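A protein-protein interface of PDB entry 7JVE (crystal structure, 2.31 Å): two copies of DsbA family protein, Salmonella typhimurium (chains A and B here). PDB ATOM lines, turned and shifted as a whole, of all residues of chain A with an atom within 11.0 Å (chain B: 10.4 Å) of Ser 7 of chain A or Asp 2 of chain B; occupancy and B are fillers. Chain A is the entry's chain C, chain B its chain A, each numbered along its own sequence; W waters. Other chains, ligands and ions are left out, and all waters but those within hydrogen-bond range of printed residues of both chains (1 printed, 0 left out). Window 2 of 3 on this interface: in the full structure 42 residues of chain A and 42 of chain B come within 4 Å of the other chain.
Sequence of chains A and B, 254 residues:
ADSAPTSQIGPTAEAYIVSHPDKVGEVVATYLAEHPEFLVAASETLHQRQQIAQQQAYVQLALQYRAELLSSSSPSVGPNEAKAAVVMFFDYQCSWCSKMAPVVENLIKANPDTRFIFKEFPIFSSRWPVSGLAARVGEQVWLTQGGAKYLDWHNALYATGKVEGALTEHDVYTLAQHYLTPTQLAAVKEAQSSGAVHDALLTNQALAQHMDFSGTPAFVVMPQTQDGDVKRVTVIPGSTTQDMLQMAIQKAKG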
ATOM      1  N   SER A   7       7.869  19.998  24.438  1.00  0.00           N
ATOM      2  CA  SER A   7       8.824  21.071  24.159  1.00  0.00           C
ATOM      3  C   SER A   7       9.599  21.489  25.418  1.00  0.00           C
ATOM      4  O   SER A   7       9.424  20.898  26.487  1.00  0.00           O
ATOM      5  CB  SER A   7       8.103  22.273  23.536  1.00  0.00           C
ATOM      6  OG  SER A   7       7.170  22.841  24.433  1.00  0.00           O
ATOM      7  N   GLN A   8      10.466  22.493  25.286  1.00  0.00           N
ATOM      8  CA  GLN A   8      11.352  22.911  26.371  1.00  0.00           C
ATOM      9  C   GLN A   8      10.691  24.026  27.173  1.00  0.00           C
ATOM     10  O   GLN A   8      10.326  25.064  26.611  1.00  0.00           O
ATOM     11  CB  GLN A   8      12.695  23.386  25.821  1.00  0.00           C
ATOM     12  CG  GLN A   8      13.469  22.351  25.020  1.00  0.00           C
ATOM     13  CD  GLN A   8      14.544  22.986  24.148  1.00  0.00           C
ATOM     14  OE1 GLN A   8      14.602  24.210  24.013  1.00  0.00           O
ATOM     15  NE2 GLN A   8      15.403  22.154  23.553  1.00  0.00           N
ATOM     16  N   ILE A   9      10.578  23.829  28.491  1.00  0.00           N
ATOM     17  CA  ILE A   9       9.796  24.742  29.325  1.00  0.00           C
ATOM     18  C   ILE A   9      10.353  26.162  29.266  1.00  0.00           C
ATOM     19  O   ILE A   9       9.606  27.128  29.081  1.00  0.00           O
ATOM     20  CB  ILE A   9       9.728  24.240  30.777  1.00  0.00           C
ATOM     21  CG1 ILE A   9       9.087  22.858  30.854  1.00  0.00           C
ATOM     22  CG2 ILE A   9       8.954  25.233  31.622  1.00  0.00           C
ATOM     23  CD1 ILE A   9       9.417  22.119  32.132  1.00  0.00           C
ATOM     24  N   GLY A  10      11.661  26.313  29.472  1.00  0.00           N
ATOM     25  CA  GLY A  10      12.275  27.618  29.565  1.00  0.00           C
ATOM     26  C   GLY A  10      11.947  28.530  28.396  1.00  0.00           C
ATOM     27  O   GLY A  10      11.364  29.608  28.564  1.00  0.00           O
ATOM     28  N   PRO A  11      12.312  28.111  27.179  1.00  0.00           N
ATOM     29  CA  PRO A  11      12.095  28.995  26.020  1.00  0.00           C
ATOM     30  C   PRO A  11      10.628  29.256  25.691  1.00  0.00           C
ATOM     31  O   PRO A  11      10.288  30.386  25.320  1.00  0.00           O
ATOM     32  CB  PRO A  11      12.820  28.261  24.877  1.00  0.00           C
ATOM     33  CG  PRO A  11      13.774  27.341  25.550  1.00  0.00           C
ATOM     34  CD  PRO A  11      13.099  26.922  26.826  1.00  0.00           C
ATOM     35  N   THR A  12       9.741  28.262  25.790  1.00  0.00           N
ATOM     36  CA  THR A  12       8.345  28.551  25.470  1.00  0.00           C
ATOM     37  C   THR A  12       7.662  29.315  26.602  1.00  0.00           C
ATOM     38  O   THR A  12       6.769  30.135  26.347  1.00  0.00           O
ATOM     39  CB  THR A  12       7.571  27.261  25.138  1.00  0.00           C
ATOM     40  OG1 THR A  12       7.415  26.455  26.313  1.00  0.00           O
ATOM     41  CG2 THR A  12       8.301  26.437  24.073  1.00  0.00           C
ATOM     42  N   ALA A  13       8.066  29.067  27.853  1.00  0.00           N
ATOM     43  CA  ALA A  13       7.567  29.871  28.960  1.00  0.00           C
ATOM     44  C   ALA A  13       7.970  31.322  28.790  1.00  0.00           C
ATOM     45  O   ALA A  13       7.201  32.239  29.108  1.00  0.00           O
ATOM     46  CB  ALA A  13       8.099  29.333  30.284  1.00  0.00           C
ATOM     47  N   GLU A  14       9.184  31.548  28.295  1.00  0.00           N
ATOM     48  CA  GLU A  14       9.670  32.904  28.088  1.00  0.00           C
ATOM     49  C   GLU A  14       8.916  33.574  26.948  1.00  0.00           C
ATOM     50  O   GLU A  14       8.453  34.712  27.078  1.00  0.00           O
ATOM     51  CB  GLU A  14      11.175  32.855  27.822  1.00  0.00           C
ATOM     52  CG  GLU A  14      11.773  34.066  27.158  1.00  0.00           C
ATOM     53  CD  GLU A  14      13.202  33.802  26.720  1.00  0.00           C
ATOM     54  OE1 GLU A  14      14.145  34.173  27.454  1.00  0.00           O
ATOM     55  OE2 GLU A  14      13.378  33.198  25.641  1.00  0.00           O
ATOM     56  N   ALA A  15       8.766  32.869  25.826  1.00  0.00           N
ATOM     57  CA  ALA A  15       7.995  33.390  24.704  1.00  0.00           C
ATOM     58  C   ALA A  15       6.588  33.802  25.125  1.00  0.00           C
ATOM     59  O   ALA A  15       6.034  34.775  24.593  1.00  0.00           O
ATOM     60  CB  ALA A  15       7.922  32.339  23.597  1.00  0.00           C
ATOM     61  N   TYR A  16       5.987  33.056  26.063  1.00  0.00           N
ATOM     62  CA  TYR A  16       4.601  33.305  26.462  1.00  0.00           C
ATOM     63  C   TYR A  16       4.485  34.559  27.326  1.00  0.00           C
ATOM     64  O   TYR A  16       3.499  35.295  27.224  1.00  0.00           O
ATOM     65  CB  TYR A  16       4.044  32.084  27.201  1.00  0.00           C
ATOM     66  CG  TYR A  16       2.591  32.197  27.633  1.00  0.00           C
ATOM     67  CD1 TYR A  16       1.566  31.750  26.807  1.00  0.00           C
ATOM     68  CD2 TYR A  16       2.249  32.738  28.868  1.00  0.00           C
ATOM     69  CE1 TYR A  16       0.243  31.838  27.192  1.00  0.00           C
ATOM     70  CE2 TYR A  16       0.923  32.832  29.266  1.00  0.00           C
ATOM     71  CZ  TYR A  16      -0.072  32.378  28.424  1.00  0.00           C
ATOM     72  OH  TYR A  16      -1.393  32.462  28.799  1.00  0.00           O
ATOM     73  N   ASP B   2       3.558  24.253  24.637  1.00  0.00           N
ATOM     74  CA  ASP B   2       3.036  22.896  24.736  1.00  0.00           C
ATOM     75  C   ASP B   2       2.831  22.513  26.218  1.00  0.00           C
ATOM     76  O   ASP B   2       2.497  23.371  27.046  1.00  0.00           O
ATOM     77  CB  ASP B   2       3.980  21.923  24.015  1.00  0.00           C
ATOM     78  CG  ASP B   2       3.371  20.540  23.805  1.00  0.00           C
ATOM     79  OD1 ASP B   2       2.128  20.425  23.712  1.00  0.00           O
ATOM     80  OD2 ASP B   2       4.144  19.564  23.713  1.00  0.00           O
ATOM     81  N   SER B   3       3.030  21.239  26.553  1.00  0.00           N
ATOM     82  CA  SER B   3       2.691  20.702  27.864  1.00  0.00           C
ATOM     83  C   SER B   3       3.922  20.071  28.512  1.00  0.00           C
ATOM     84  O   SER B   3       4.909  19.751  27.842  1.00  0.00           O
ATOM     85  CB  SER B   3       1.547  19.674  27.748  1.00  0.00           C
ATOM     86  OG  SER B   3       1.042  19.293  29.016  1.00  0.00           O
ATOM     87  N   ALA B   4       3.850  19.891  29.839  1.00  0.00           N
ATOM     88  CA  ALA B   4       4.974  19.402  30.635  1.00  0.00           C
ATOM     89  C   ALA B   4       4.551  19.142  32.080  1.00  0.00           C
ATOM     90  O   ALA B   4       3.449  19.538  32.484  1.00  0.00           O
ATOM     91  CB  ALA B   4       6.133  20.405  30.597  1.00  0.00           C
ATOM     92  N   PRO B   5       5.389  18.489  32.887  1.00  0.00           N
ATOM     93  CA  PRO B   5       5.017  18.222  34.284  1.00  0.00           C
ATOM     94  C   PRO B   5       4.770  19.508  35.062  1.00  0.00           C
ATOM     95  O   PRO B   5       5.618  20.405  35.105  1.00  0.00           O
ATOM     96  CB  PRO B   5       6.224  17.453  34.828  1.00  0.00           C
ATOM     97  CG  PRO B   5       6.805  16.794  33.613  1.00  0.00           C
ATOM     98  CD  PRO B   5       6.643  17.810  32.519  1.00  0.00           C
ATOM     99  N   THR B   6       3.602  19.567  35.709  1.00  0.00           N
ATOM    100  CA  THR B   6       3.177  20.777  36.405  1.00  0.00           C
ATOM    101  C   THR B   6       4.174  21.195  37.476  1.00  0.00           C
ATOM    102  O   THR B   6       4.511  22.379  37.596  1.00  0.00           O
ATOM    103  CB  THR B   6       1.797  20.549  37.023  1.00  0.00           C
ATOM    104  OG1 THR B   6       0.836  20.427  35.973  1.00  0.00           O
ATOM    105  CG2 THR B   6       1.421  21.696  37.940  1.00  0.00           C
ATOM    106  N   GLN B   8       7.261  20.907  37.607  1.00  0.00           N
ATOM    107  CA  GLN B   8       8.539  21.398  37.091  1.00  0.00           C
ATOM    108  C   GLN B   8       8.426  22.704  36.315  1.00  0.00           C
ATOM    109  O   GLN B   8       9.438  23.395  36.142  1.00  0.00           O
ATOM    110  CB  GLN B   8       9.203  20.355  36.177  1.00  0.00           C
ATOM    111  CG  GLN B   8       9.549  19.055  36.848  1.00  0.00           C
ATOM    112  CD  GLN B   8      10.080  18.025  35.866  1.00  0.00           C
ATOM    113  OE1 GLN B   8      10.147  18.271  34.660  1.00  0.00           O
ATOM    114  NE2 GLN B   8      10.460  16.864  36.380  1.00  0.00           N
ATOM    115  N   ILE B   9       7.233  23.061  35.848  1.00  0.00           N
ATOM    116  CA  ILE B   9       7.122  24.190  34.934  1.00  0.00           C
ATOM    117  C   ILE B   9       7.546  25.484  35.621  1.00  0.00           C
ATOM    118  O   ILE B   9       8.419  26.213  35.135  1.00  0.00           O
ATOM    119  CB  ILE B   9       5.694  24.298  34.386  1.00  0.00           C
ATOM    120  CG1 ILE B   9       5.367  23.031  33.601  1.00  0.00           C
ATOM    121  CG2 ILE B   9       5.555  25.595  33.561  1.00  0.00           C
ATOM    122  CD1 ILE B   9       3.914  22.901  33.211  1.00  0.00           C
ATOM    123  N   THR B  12      11.217  25.766  36.693  1.00  0.00           N
ATOM    124  CA  THR B  12      12.090  25.748  35.523  1.00  0.00           C
ATOM    125  C   THR B  12      11.959  27.040  34.726  1.00  0.00           C
ATOM    126  O   THR B  12      12.964  27.626  34.302  1.00  0.00           O
ATOM    127  CB  THR B  12      11.783  24.521  34.652  1.00  0.00           C
ATOM    128  OG1 THR B  12      12.075  23.316  35.379  1.00  0.00           O
ATOM    129  CG2 THR B  12      12.624  24.519  33.376  1.00  0.00           C
ATOM    130  N   TYR B  16      15.072  29.616  34.069  1.00  0.00           N
ATOM    131  CA  TYR B  16      15.510  29.943  32.719  1.00  0.00           C
ATOM    132  C   TYR B  16      15.607  31.457  32.533  1.00  0.00           C
ATOM    133  O   TYR B  16      16.594  31.962  31.984  1.00  0.00           O
ATOM    134  CB  TYR B  16      14.562  29.310  31.690  1.00  0.00           C
ATOM    135  CG  TYR B  16      15.007  29.516  30.254  1.00  0.00           C
ATOM    136  CD1 TYR B  16      14.651  30.668  29.556  1.00  0.00           C
ATOM    137  CD2 TYR B  16      15.797  28.572  29.599  1.00  0.00           C
ATOM    138  CE1 TYR B  16      15.055  30.879  28.255  1.00  0.00           C
ATOM    139  CE2 TYR B  16      16.209  28.772  28.278  1.00  0.00           C
ATOM    140  CZ  TYR B  16      15.830  29.936  27.621  1.00  0.00           C
ATOM    141  OH  TYR B  16      16.220  30.171  26.327  1.00  0.00           O
HETATM  142  O   HOH W   1      16.703  33.089  25.069  1.00  0.00           O
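Of the printed residues of chain B, Ser 7 of chain A touches Asp 2 (3.3 Å).
No residue of chain B comes within 4 Å of Gln 8 of chain A.
Of the printed residues of chain B, Pro 11 of chain A touches Tyr 16.
Printed residues of chain B within 4 Å of Glu 14 of chain A: Tyr 16.
No residue of chain A comes within 4 Å of Ser 3 of chain B.
Ala 4 of chain B touches one residue of chain A.
Pro 5 of chain B touches none of the printed residues of chain A.
Thr 6 of chain B touches none of the printed residues of chain A.
Of the printed residues of chain A, Ile 9 of chain B touches Ile 9.
Of the printed residues of chain A, Tyr 16 of chain B touches Gly 10, Pro 11 and Glu 14.
The nearest residue of chain B that does not touch Ser 7 of chain A is Ser 3 of chain B (4.5 Å).
The nearest printed residue of chain A that does not touch Thr 12 of chain B is Gly 10 of chain A (4.4 Å).
O of Gln 8 of chain B lies within hydrogen-bond range of OG1 of Thr 12 of chain B (2.7 Å).
Ile 9 of chain A touches its own counterpart, Ile 9 of chain B.
Ile 9 of chain A touches Thr 12 of chain B, but with the chains exchanged Thr 12 of chain A does not touch Ile 9 of chain B (7.5 Å).
Positions printed for both chains: 8, 9, 12 and 16.
Of the 9 printed residues of chain B, 5 touch a printed residue of chain A.
Among the printed residues, no Asp or Glu carboxylate lies within 4 Å of a Lys or Arg side-chain nitrogen of the other chain.
Ser 7 of chain A touches Asp 2 of chain B.
CG1 of Ile 9 of chain A touches CB of Ala 4 of chain B (3.8 Å).
Ile 9 of chain A touches Ile 9 of chain B.
Ile 9 of chain A touches Thr 12 of chain B (CB to CG2, 3.9 Å).
CA of Gly 10 of chain A touches CG of Tyr 16 of chain B, at 3.4 Å.
CG of Pro 11 of chain A touches OH of Tyr 16 of chain B, 3.8 Å away.
Tyr 16 of chain B touches Glu 14 of chain A.
Water W1 bridges OH of Tyr 16 of chain B (3.2 Å) and OE2 of Glu 14 of chain A (3.4 Å).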
